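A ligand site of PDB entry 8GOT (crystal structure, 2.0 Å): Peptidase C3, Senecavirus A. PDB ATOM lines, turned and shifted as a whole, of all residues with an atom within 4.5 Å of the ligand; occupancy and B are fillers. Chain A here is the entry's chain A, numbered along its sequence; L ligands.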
ATOM      1  N   GLU A  47      20.282  -9.771   7.197  1.00  0.00           N
ATOM      2  CA  GLU A  47      20.372  -8.987   8.425  1.00  0.00           C
ATOM      3  C   GLU A  47      20.610  -9.887   9.627  1.00  0.00           C
ATOM      4  O   GLU A  47      21.381  -9.523  10.525  1.00  0.00           O
ATOM      5  CB  GLU A  47      19.109  -8.153   8.630  1.00  0.00           C
ATOM      6  CG  GLU A  47      19.124  -7.234   9.868  1.00  0.00           C
ATOM      7  CD  GLU A  47      18.657  -7.931  11.149  1.00  0.00           C
ATOM      8  OE1 GLU A  47      18.026  -9.000  11.068  1.00  0.00           O
ATOM      9  OE2 GLU A  47      18.933  -7.393  12.243  1.00  0.00           O
ATOM     10  N   PRO A  70      35.020  -0.080  10.569  1.00  0.00           N
ATOM     11  CA  PRO A  70      33.943   0.917  10.414  1.00  0.00           C
ATOM     12  C   PRO A  70      33.114   0.687   9.151  1.00  0.00           C
ATOM     13  O   PRO A  70      33.125   1.481   8.201  1.00  0.00           O
ATOM     14  CB  PRO A  70      34.723   2.223  10.353  1.00  0.00           C
ATOM     15  CG  PRO A  70      35.954   1.844   9.608  1.00  0.00           C
ATOM     16  CD  PRO A  70      36.319   0.462  10.109  1.00  0.00           C
ATOM     17  N   PHE A  71      32.373  -0.420   9.113  1.00  0.00           N
ATOM     18  CA  PHE A  71      31.542  -0.665   7.944  1.00  0.00           C
ATOM     19  C   PHE A  71      30.435   0.380   7.844  1.00  0.00           C
ATOM     20  O   PHE A  71      29.823   0.759   8.844  1.00  0.00           O
ATOM     21  CB  PHE A  71      30.900  -2.048   8.002  1.00  0.00           C
ATOM     22  CG  PHE A  71      31.821  -3.153   8.393  1.00  0.00           C
ATOM     23  CD1 PHE A  71      32.700  -3.722   7.472  1.00  0.00           C
ATOM     24  CD2 PHE A  71      31.796  -3.666   9.685  1.00  0.00           C
ATOM     25  CE1 PHE A  71      33.540  -4.760   7.833  1.00  0.00           C
ATOM     26  CE2 PHE A  71      32.620  -4.706  10.052  1.00  0.00           C
ATOM     27  CZ  PHE A  71      33.496  -5.250   9.128  1.00  0.00           C
ATOM     28  N   GLN A  72      30.172   0.837   6.626  1.00  0.00           N
ATOM     29  CA  GLN A  72      28.955   1.587   6.354  1.00  0.00           C
ATOM     30  C   GLN A  72      27.878   0.592   5.942  1.00  0.00           C
ATOM     31  O   GLN A  72      28.094  -0.231   5.042  1.00  0.00           O
ATOM     32  CB  GLN A  72      29.173   2.629   5.272  1.00  0.00           C
ATOM     33  CG  GLN A  72      30.540   3.268   5.247  1.00  0.00           C
ATOM     34  CD  GLN A  72      30.606   4.474   4.331  1.00  0.00           C
ATOM     35  OE1 GLN A  72      29.722   5.339   4.345  1.00  0.00           O
ATOM     36  NE2 GLN A  72      31.651   4.548   3.512  1.00  0.00           N
ATOM     37  N   THR A  73      26.724   0.645   6.602  1.00  0.00           N
ATOM     38  CA  THR A  73      25.679  -0.328   6.341  1.00  0.00           C
ATOM     39  C   THR A  73      24.325   0.345   6.212  1.00  0.00           C
ATOM     40  O   THR A  73      24.057   1.395   6.797  1.00  0.00           O
ATOM     41  CB  THR A  73      25.571  -1.382   7.450  1.00  0.00           C
ATOM     42  OG1 THR A  73      25.055  -0.778   8.645  1.00  0.00           O
ATOM     43  CG2 THR A  73      26.919  -2.050   7.702  1.00  0.00           C
ATOM     44  N   VAL A  74      23.450  -0.292   5.431  1.00  0.00           N
ATOM     45  CA  VAL A  74      22.063   0.092   5.300  1.00  0.00           C
ATOM     46  C   VAL A  74      21.205  -1.128   5.606  1.00  0.00           C
ATOM     47  O   VAL A  74      21.420  -2.199   5.019  1.00  0.00           O
ATOM     48  CB  VAL A  74      21.753   0.641   3.894  1.00  0.00           C
ATOM     49  CG1 VAL A  74      20.251   0.831   3.719  1.00  0.00           C
ATOM     50  CG2 VAL A  74      22.496   1.949   3.679  1.00  0.00           C
ATOM     51  N   HIS A  75      20.258  -0.975   6.521  1.00  0.00           N
ATOM     52  CA  HIS A  75      19.279  -1.996   6.850  1.00  0.00           C
ATOM     53  C   HIS A  75      17.935  -1.566   6.281  1.00  0.00           C
ATOM     54  O   HIS A  75      17.410  -0.519   6.659  1.00  0.00           O
ATOM     55  CB  HIS A  75      19.201  -2.206   8.358  1.00  0.00           C
ATOM     56  CG  HIS A  75      18.130  -3.184   8.755  1.00  0.00           C
ATOM     57  ND1 HIS A  75      17.433  -3.085   9.943  1.00  0.00           N
ATOM     58  CD2 HIS A  75      17.645  -4.275   8.117  1.00  0.00           C
ATOM     59  CE1 HIS A  75      16.557  -4.072  10.014  1.00  0.00           C
ATOM     60  NE2 HIS A  75      16.658  -4.810   8.926  1.00  0.00           N
ATOM     61  N   PHE A  76      17.390  -2.361   5.365  1.00  0.00           N
ATOM     62  CA  PHE A  76      16.131  -1.980   4.724  1.00  0.00           C
ATOM     63  C   PHE A  76      14.941  -2.318   5.620  1.00  0.00           C
ATOM     64  O   PHE A  76      14.899  -3.358   6.274  1.00  0.00           O
ATOM     65  CB  PHE A  76      16.005  -2.670   3.357  1.00  0.00           C
ATOM     66  CG  PHE A  76      17.032  -2.218   2.337  1.00  0.00           C
ATOM     67  CD1 PHE A  76      16.795  -1.115   1.539  1.00  0.00           C
ATOM     68  CD2 PHE A  76      18.243  -2.880   2.219  1.00  0.00           C
ATOM     69  CE1 PHE A  76      17.737  -0.686   0.620  1.00  0.00           C
ATOM     70  CE2 PHE A  76      19.192  -2.458   1.299  1.00  0.00           C
ATOM     71  CZ  PHE A  76      18.933  -1.359   0.493  1.00  0.00           C
ATOM     72  N   THR A  77      13.960  -1.406   5.636  1.00  0.00           N
ATOM     73  CA  THR A  77      12.704  -1.604   6.357  1.00  0.00           C
ATOM     74  C   THR A  77      11.541  -1.377   5.393  1.00  0.00           C
ATOM     75  O   THR A  77      11.688  -0.759   4.344  1.00  0.00           O
ATOM     76  CB  THR A  77      12.562  -0.660   7.560  1.00  0.00           C
ATOM     77  OG1 THR A  77      12.579   0.698   7.102  1.00  0.00           O
ATOM     78  CG2 THR A  77      13.678  -0.881   8.569  1.00  0.00           C
ATOM     79  N   HIS A  78      10.375  -1.881   5.773  1.00  0.00           N
ATOM     80  CA  HIS A  78       9.158  -1.714   4.980  1.00  0.00           C
ATOM     81  C   HIS A  78       8.012  -1.391   5.918  1.00  0.00           C
ATOM     82  O   HIS A  78       7.656  -2.202   6.774  1.00  0.00           O
ATOM     83  CB  HIS A  78       8.853  -2.968   4.151  1.00  0.00           C
ATOM     84  CG  HIS A  78       7.825  -2.739   3.081  1.00  0.00           C
ATOM     85  ND1 HIS A  78       8.064  -1.972   1.962  1.00  0.00           N
ATOM     86  CD2 HIS A  78       6.544  -3.185   2.962  1.00  0.00           C
ATOM     87  CE1 HIS A  78       6.985  -1.942   1.199  1.00  0.00           C
ATOM     88  NE2 HIS A  78       6.043  -2.678   1.784  1.00  0.00           N
ATOM     89  N   HIS A  79       7.432  -0.195   5.738  1.00  0.00           N
ATOM     90  CA  HIS A  79       6.316   0.279   6.565  1.00  0.00           C
ATOM     91  C   HIS A  79       6.628   0.114   8.058  1.00  0.00           C
ATOM     92  O   HIS A  79       5.765  -0.279   8.847  1.00  0.00           O
ATOM     93  CB  HIS A  79       4.996  -0.429   6.208  1.00  0.00           C
ATOM     94  CG  HIS A  79       4.548  -0.208   4.789  1.00  0.00           C
ATOM     95  ND1 HIS A  79       5.162   0.674   3.933  1.00  0.00           N
ATOM     96  CD2 HIS A  79       3.516  -0.756   4.099  1.00  0.00           C
ATOM     97  CE1 HIS A  79       4.548   0.655   2.760  1.00  0.00           C
ATOM     98  NE2 HIS A  79       3.545  -0.203   2.835  1.00  0.00           N
ATOM     99  N   PRO A  82      11.213  -4.385  10.059  1.00  0.00           N
ATOM    100  CA  PRO A  82      12.511  -4.752   9.470  1.00  0.00           C
ATOM    101  C   PRO A  82      12.380  -5.812   8.378  1.00  0.00           C
ATOM    102  O   PRO A  82      11.543  -6.724   8.467  1.00  0.00           O
ATOM    103  CB  PRO A  82      13.289  -5.295  10.668  1.00  0.00           C
ATOM    104  CG  PRO A  82      12.236  -5.699  11.665  1.00  0.00           C
ATOM    105  CD  PRO A  82      11.151  -4.679  11.494  1.00  0.00           C
ATOM    106  N   GLN A 142      13.255 -15.721  14.809  1.00  0.00           N
ATOM    107  CA  GLN A 142      13.929 -14.498  15.242  1.00  0.00           C
ATOM    108  C   GLN A 142      13.034 -13.270  15.018  1.00  0.00           C
ATOM    109  O   GLN A 142      13.527 -12.165  14.807  1.00  0.00           O
ATOM    110  CB  GLN A 142      15.274 -14.330  14.534  1.00  0.00           C
ATOM    111  CG  GLN A 142      16.241 -15.483  14.797  1.00  0.00           C
ATOM    112  CD  GLN A 142      17.592 -15.301  14.130  1.00  0.00           C
ATOM    113  OE1 GLN A 142      18.141 -14.194  14.080  1.00  0.00           O
ATOM    114  NE2 GLN A 142      18.129 -16.398  13.591  1.00  0.00           N
ATOM    115  N   TYR A 145       9.671 -10.604   9.899  1.00  0.00           N
ATOM    116  CA  TYR A 145      10.443  -9.920   8.866  1.00  0.00           C
ATOM    117  C   TYR A 145       9.524  -9.567   7.709  1.00  0.00           C
ATOM    118  O   TYR A 145       8.558 -10.288   7.426  1.00  0.00           O
ATOM    119  CB  TYR A 145      11.607 -10.788   8.352  1.00  0.00           C
ATOM    120  CG  TYR A 145      12.804 -10.869   9.273  1.00  0.00           C
ATOM    121  CD1 TYR A 145      13.696  -9.812   9.390  1.00  0.00           C
ATOM    122  CD2 TYR A 145      13.056 -12.021  10.022  1.00  0.00           C
ATOM    123  CE1 TYR A 145      14.798  -9.898  10.215  1.00  0.00           C
ATOM    124  CE2 TYR A 145      14.156 -12.111  10.856  1.00  0.00           C
ATOM    125  CZ  TYR A 145      15.025 -11.044  10.949  1.00  0.00           C
ATOM    126  OH  TYR A 145      16.132 -11.110  11.761  1.00  0.00           O
ATOM    127  N   SER A 192      14.721  -4.427  -4.697  1.00  0.00           N
ATOM    128  CA  SER A 192      14.322  -3.540  -5.783  1.00  0.00           C
ATOM    129  C   SER A 192      15.514  -2.716  -6.240  1.00  0.00           C
ATOM    130  O   SER A 192      16.403  -2.379  -5.452  1.00  0.00           O
ATOM    131  CB  SER A 192      13.164  -2.623  -5.392  1.00  0.00           C
ATOM    132  OG  SER A 192      13.589  -1.541  -4.597  1.00  0.00           O
ATOM    133  N   LEU A 194      15.414   0.382  -7.264  1.00  0.00           N
ATOM    134  CA  LEU A 194      15.323   1.716  -6.671  1.00  0.00           C
ATOM    135  C   LEU A 194      15.878   1.728  -5.251  1.00  0.00           C
ATOM    136  O   LEU A 194      16.598   2.661  -4.876  1.00  0.00           O
ATOM    137  CB  LEU A 194      13.874   2.191  -6.684  1.00  0.00           C
ATOM    138  CG  LEU A 194      13.592   3.262  -7.741  1.00  0.00           C
ATOM    139  CD1 LEU A 194      14.090   2.818  -9.123  1.00  0.00           C
ATOM    140  CD2 LEU A 194      12.102   3.568  -7.788  1.00  0.00           C
ATOM    141  N   GLY A 195      15.562   0.692  -4.461  1.00  0.00           N
ATOM    142  CA  GLY A 195      16.147   0.595  -3.131  1.00  0.00           C
ATOM    143  C   GLY A 195      17.658   0.495  -3.163  1.00  0.00           C
ATOM    144  O   GLY A 195      18.357   1.165  -2.398  1.00  0.00           O
ATOM    145  N   ILE A 197      19.702   1.567  -5.505  1.00  0.00           N
ATOM    146  CA  ILE A 197      20.299   2.815  -5.964  1.00  0.00           C
ATOM    147  C   ILE A 197      20.374   3.832  -4.838  1.00  0.00           C
ATOM    148  O   ILE A 197      21.386   4.527  -4.663  1.00  0.00           O
ATOM    149  CB  ILE A 197      19.513   3.366  -7.182  1.00  0.00           C
ATOM    150  CG1 ILE A 197      19.665   2.445  -8.384  1.00  0.00           C
ATOM    151  CG2 ILE A 197      19.938   4.793  -7.507  1.00  0.00           C
ATOM    152  CD1 ILE A 197      21.071   2.359  -8.919  1.00  0.00           C
ATOM    153  N   LYS A 198      19.300   3.941  -4.054  1.00  0.00           N
ATOM    154  CA  LYS A 198      19.261   4.946  -3.009  1.00  0.00           C
ATOM    155  C   LYS A 198      20.146   4.532  -1.831  1.00  0.00           C
ATOM    156  O   LYS A 198      20.746   5.385  -1.176  1.00  0.00           O
ATOM    157  CB  LYS A 198      17.819   5.175  -2.561  1.00  0.00           C
ATOM    158  CG  LYS A 198      17.598   5.479  -1.090  1.00  0.00           C
ATOM    159  CD  LYS A 198      16.158   5.944  -0.870  1.00  0.00           C
ATOM    160  CE  LYS A 198      15.453   5.189   0.243  1.00  0.00           C
ATOM    161  NZ  LYS A 198      14.222   5.909   0.691  1.00  0.00           N
ATOM    162  N   HIS A 202      23.442   6.640  -0.311  1.00  0.00           N
ATOM    163  CA  HIS A 202      23.626   6.884   1.119  1.00  0.00           C
ATOM    164  C   HIS A 202      24.995   6.384   1.577  1.00  0.00           C
ATOM    165  O   HIS A 202      25.656   7.055   2.377  1.00  0.00           O
ATOM    166  CB  HIS A 202      22.478   6.219   1.897  1.00  0.00           C
ATOM    167  CG  HIS A 202      22.554   6.344   3.382  1.00  0.00           C
ATOM    168  ND1 HIS A 202      21.433   6.339   4.185  1.00  0.00           N
ATOM    169  CD2 HIS A 202      23.596   6.430   4.236  1.00  0.00           C
ATOM    170  CE1 HIS A 202      21.763   6.440   5.454  1.00  0.00           C
ATOM    171  NE2 HIS A 202      23.085   6.495   5.519  1.00  0.00           N
ATOM    172  N   THR A 209      25.698   8.596 -13.060  1.00  0.00           N
ATOM    173  CA  THR A 209      24.269   8.520 -13.297  1.00  0.00           C
ATOM    174  C   THR A 209      24.007   8.677 -14.790  1.00  0.00           C
ATOM    175  O   THR A 209      24.501   9.622 -15.420  1.00  0.00           O
ATOM    176  CB  THR A 209      23.508   9.579 -12.481  1.00  0.00           C
ATOM    177  OG1 THR A 209      23.739   9.340 -11.085  1.00  0.00           O
ATOM    178  CG2 THR A 209      22.034   9.524 -12.767  1.00  0.00           C
HETATM  179  C1  LIG L   1       7.302   1.512  -1.524  1.00  0.00           C
HETATM  180  O1  LIG L   1      11.377   2.486  -0.444  1.00  0.00           O
HETATM  181  C2  LIG L   1      11.764   2.441  -1.810  1.00  0.00           C
HETATM  182  C3  LIG L   1      11.712   1.099  -2.602  1.00  0.00           C
HETATM  183  P1  LIG L   1       9.701   2.471   3.592  1.00  0.00           P
HETATM  184  O2  LIG L   1       9.424   3.930   3.313  1.00  0.00           O
HETATM  185  O3  LIG L   1      11.319   2.271   3.918  1.00  0.00           O
HETATM  186  O4  LIG L   1       8.697   1.964   4.273  1.00  0.00           O
HETATM  187  C4  LIG L   1      12.249   3.104   3.244  1.00  0.00           C
HETATM  188  C5  LIG L   1      13.280   2.192   2.563  1.00  0.00           C
HETATM  189  C6  LIG L   1      14.184   1.575   3.656  1.00  0.00           C
HETATM  190  C7  LIG L   1       6.045   1.799  -2.369  1.00  0.00           C
HETATM  191  O5  LIG L   1       7.636   0.386  -1.320  1.00  0.00           O
HETATM  192  O6  LIG L   1       8.046   2.582  -0.999  1.00  0.00           O
HETATM  193  O7  LIG L   1      12.143   3.422  -2.370  1.00  0.00           O
HETATM  194  C8  LIG L   1       9.027   2.221  -0.072  1.00  0.00           C
HETATM  195  C9  LIG L   1      10.183   3.226  -0.201  1.00  0.00           C
HETATM  196  O8  LIG L   1      12.600   1.160   1.882  1.00  0.00           O
HETATM  197  O9  LIG L   1      14.626   2.639   4.494  1.00  0.00           O
HETATM  198  P2  LIG L   1      16.270   2.842   4.631  1.00  0.00           P
HETATM  199  O10 LIG L   1      16.680   4.238   4.233  1.00  0.00           O
HETATM  200  C10 LIG L   1       8.409   2.280   1.345  1.00  0.00           C
HETATM  201  O11 LIG L   1      17.015   2.502   3.339  1.00  0.00           O
HETATM  202  O12 LIG L   1       9.263   1.600   2.253  1.00  0.00           O
HETATM  203  O13 LIG L   1      16.695   2.591   6.221  1.00  0.00           O
HETATM  204  C11 LIG L   1      17.307   3.651   6.928  1.00  0.00           C
HETATM  205  C12 LIG L   1      18.201   2.978   7.973  1.00  0.00           C
HETATM  206  C13 LIG L   1      19.500   2.573   7.269  1.00  0.00           C
HETATM  207  O14 LIG L   1      20.359   1.961   8.217  1.00  0.00           O
HETATM  208  C14 LIG L   1      21.307   2.895   8.713  1.00  0.00           C
HETATM  209  C15 LIG L   1      21.716   2.861  10.197  1.00  0.00           C
HETATM  210  O15 LIG L   1      21.767   3.715   7.979  1.00  0.00           O
HETATM  211  O16 LIG L   1      17.570   1.804   8.362  1.00  0.00           O
HETATM  212  C16 LIG L   1      16.811   1.885   9.558  1.00  0.00           C
HETATM  213  C17 LIG L   1      17.511   1.657  10.925  1.00  0.00           C
HETATM  214  O17 LIG L   1      15.657   2.130   9.516  1.00  0.00           O
HETATM  215  C18 LIG L   1       5.225   2.974  -1.802  1.00  0.00           C
HETATM  216  C19 LIG L   1       4.565   2.594  -0.449  1.00  0.00           C
HETATM  217  C20 LIG L   1       4.364   3.807   0.487  1.00  0.00           C
HETATM  218  C21 LIG L   1       2.928   3.874   1.051  1.00  0.00           C
HETATM  219  C22 LIG L   1       1.878   4.326  -0.003  1.00  0.00           C
HETATM  220  C23 LIG L   1       0.725   3.309  -0.168  1.00  0.00           C
HETATM  221  C24 LIG L   1       0.813   2.540  -1.518  1.00  0.00           C
HETATM  222  C25 LIG L   1       1.156   3.185  -2.644  1.00  0.00           C
HETATM  223  C26 LIG L   1       1.239   2.408  -3.975  1.00  0.00           C
HETATM  224  C27 LIG L   1       2.244   1.234  -3.910  1.00  0.00           C
HETATM  225  C28 LIG L   1       2.448   0.465  -4.981  1.00  0.00           C
HETATM  226  C29 LIG L   1       1.681   0.760  -6.284  1.00  0.00           C
HETATM  227  C30 LIG L   1       1.162  -0.533  -6.968  1.00  0.00           C
HETATM  228  C31 LIG L   1       1.665  -0.675  -8.439  1.00  0.00           C
HETATM  229  C32 LIG L   1       0.496  -0.759  -9.463  1.00  0.00           C
HETATM  230  C33 LIG L   1       0.432  -2.120 -10.188  1.00  0.00           C
HETATM  231  C34 LIG L   1      11.280   1.356  -4.071  1.00  0.00           C
HETATM  232  C35 LIG L   1       9.781   1.003  -4.337  1.00  0.00           C
HETATM  233  C36 LIG L   1       8.968   2.213  -4.879  1.00  0.00           C
HETATM  234  C37 LIG L   1       9.215   3.452  -4.427  1.00  0.00           C
HETATM  235  C38 LIG L   1       8.391   4.639  -4.970  1.00  0.00           C
HETATM  236  C39 LIG L   1       9.087   5.381  -6.146  1.00  0.00           C
HETATM  237  C40 LIG L   1      10.005   6.334  -5.885  1.00  0.00           C
HETATM  238  C41 LIG L   1      10.708   7.082  -7.057  1.00  0.00           C
HETATM  239  C42 LIG L   1      10.115   6.689  -8.439  1.00  0.00           C
HETATM  240  C43 LIG L   1      10.873   6.784  -9.544  1.00  0.00           C
HETATM  241  C44 LIG L   1      12.330   7.283  -9.431  1.00  0.00           C
HETATM  242  C45 LIG L   1      13.301   6.482 -10.330  1.00  0.00           C
HETATM  243  C46 LIG L   1      14.615   6.720 -10.262  1.00  0.00           C
HETATM  244  C47 LIG L   1      15.593   5.912 -11.161  1.00  0.00           C
HETATM  245  C48 LIG L   1      16.883   5.514 -10.384  1.00  0.00           C
HETATM  246  C49 LIG L   1      17.514   6.726  -9.656  1.00  0.00           C
HETATM  247  C50 LIG L   1      18.816   7.206 -10.341  1.00  0.00           C
HETATM  248  C51 LIG L   1      19.568   8.269  -9.516  1.00  0.00           C
HETATM  249  C52 LIG L   1      23.019   2.035  10.407  1.00  0.00           C
HETATM  250  C53 LIG L   1      24.246   2.956  10.676  1.00  0.00           C
HETATM  251  C54 LIG L   1      25.557   2.153  10.865  1.00  0.00           C
HETATM  252  C55 LIG L   1      26.502   2.286   9.639  1.00  0.00           C
HETATM  253  C56 LIG L   1      26.512   3.713   9.029  1.00  0.00           C
HETATM  254  C57 LIG L   1      27.565   4.617   9.744  1.00  0.00           C
HETATM  255  C58 LIG L   1      29.005   4.252   9.297  1.00  0.00           C
HETATM  256  C59 LIG L   1      29.937   3.892  10.488  1.00  0.00           C
HETATM  257  C60 LIG L   1      31.411   4.125  10.065  1.00  0.00           C
HETATM  258  C61 LIG L   1      31.444   4.563   8.579  1.00  0.00           C
HETATM  259  C62 LIG L   1      32.815   5.119   8.099  1.00  0.00           C
HETATM  260  C63 LIG L   1      32.615   6.356   7.176  1.00  0.00           C
HETATM  261  C64 LIG L   1      31.288   7.090   7.479  1.00  0.00           C
HETATM  262  C65 LIG L   1      30.984   8.253   6.497  1.00  0.00           C
HETATM  263  C66 LIG L   1      29.461   8.446   6.262  1.00  0.00           C
HETATM  264  C67 LIG L   1      28.595   7.482   7.124  1.00  0.00           C
HETATM  265  C68 LIG L   1      27.221   7.174   6.477  1.00  0.00           C
HETATM  266  C69 LIG L   1      26.649   8.413   5.737  1.00  0.00           C
HETATM  267  C70 LIG L   1      17.867   0.170  11.137  1.00  0.00           C
HETATM  268  C71 LIG L   1      17.048  -0.439  12.309  1.00  0.00           C
HETATM  269  C72 LIG L   1      15.533  -0.489  12.013  1.00  0.00           C
HETATM  270  C73 LIG L   1      14.893  -1.859  12.378  1.00  0.00           C
HETATM  271  C74 LIG L   1      14.075  -2.441  13.561  1.00  0.00           C
HETATM  272  C75 LIG L   1      14.690  -3.723  14.195  1.00  0.00           C
HETATM  273  C76 LIG L   1      15.985  -4.210  13.469  1.00  0.00           C
HETATM  274  C77 LIG L   1      16.193  -5.745  13.542  1.00  0.00           C
HETATM  275  C78 LIG L   1      15.583  -7.031  12.902  1.00  0.00           C
HETATM  276  C79 LIG L   1      14.651  -7.847  13.837  1.00  0.00           C
HETATM  277  C80 LIG L   1      15.335  -8.223  15.174  1.00  0.00           C
HETATM  278  C81 LIG L   1      14.636  -7.558  16.396  1.00  0.00           C
HETATM  279  C82 LIG L   1      15.654  -6.926  17.372  1.00  0.00           C
HETATM  280  C83 LIG L   1      15.272  -5.478  17.771  1.00  0.00           C
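O14 of the ligand sits at hydrogen-bond distance from N of His 75 (3.4 Å). O4 of the ligand is in hydrogen-bond range of N of His 79, at 2.9 Å. The backbone carbonyl oxygen of Thr 77 lies within hydrogen-bond range of an oxygen (O8) of the ligand, at 3.3 Å.
OE1 of Glu 47 sits at hydrogen-bond distance from OH of Tyr 145 (2.9 Å). The side-chain hydroxyl (OG) of Ser 192 is in hydrogen-bond range of the backbone NH (N) of Gly 195, at 3.0 Å.
O of Thr 73 sits close to O15 of the ligand, 3.5 Å away. Merely in contact with the ligand: Glu 47, His 78, Pro 70, Phe 71, Pro 82, Gln 72, Val 74, His 202, Ser 192, Leu 194 and Ile 197. Hydrophobic or aromatic side chains within 4 Å of the ligand: Pro 70, Val 74, His 75, His 78, His 79, Pro 82, Leu 194, Ile 197 and His 202. Within 4 Å of the ligand: Glu 47, Pro 70, Phe 71, Gln 72, Thr 73, Val 74, His 75, Thr 77, His 78, His 79, Pro 82, Ser 192, Leu 194, Ile 197 and His 202. Along chain A the residues within 4 Å of the ligand span positions 47 to 202.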
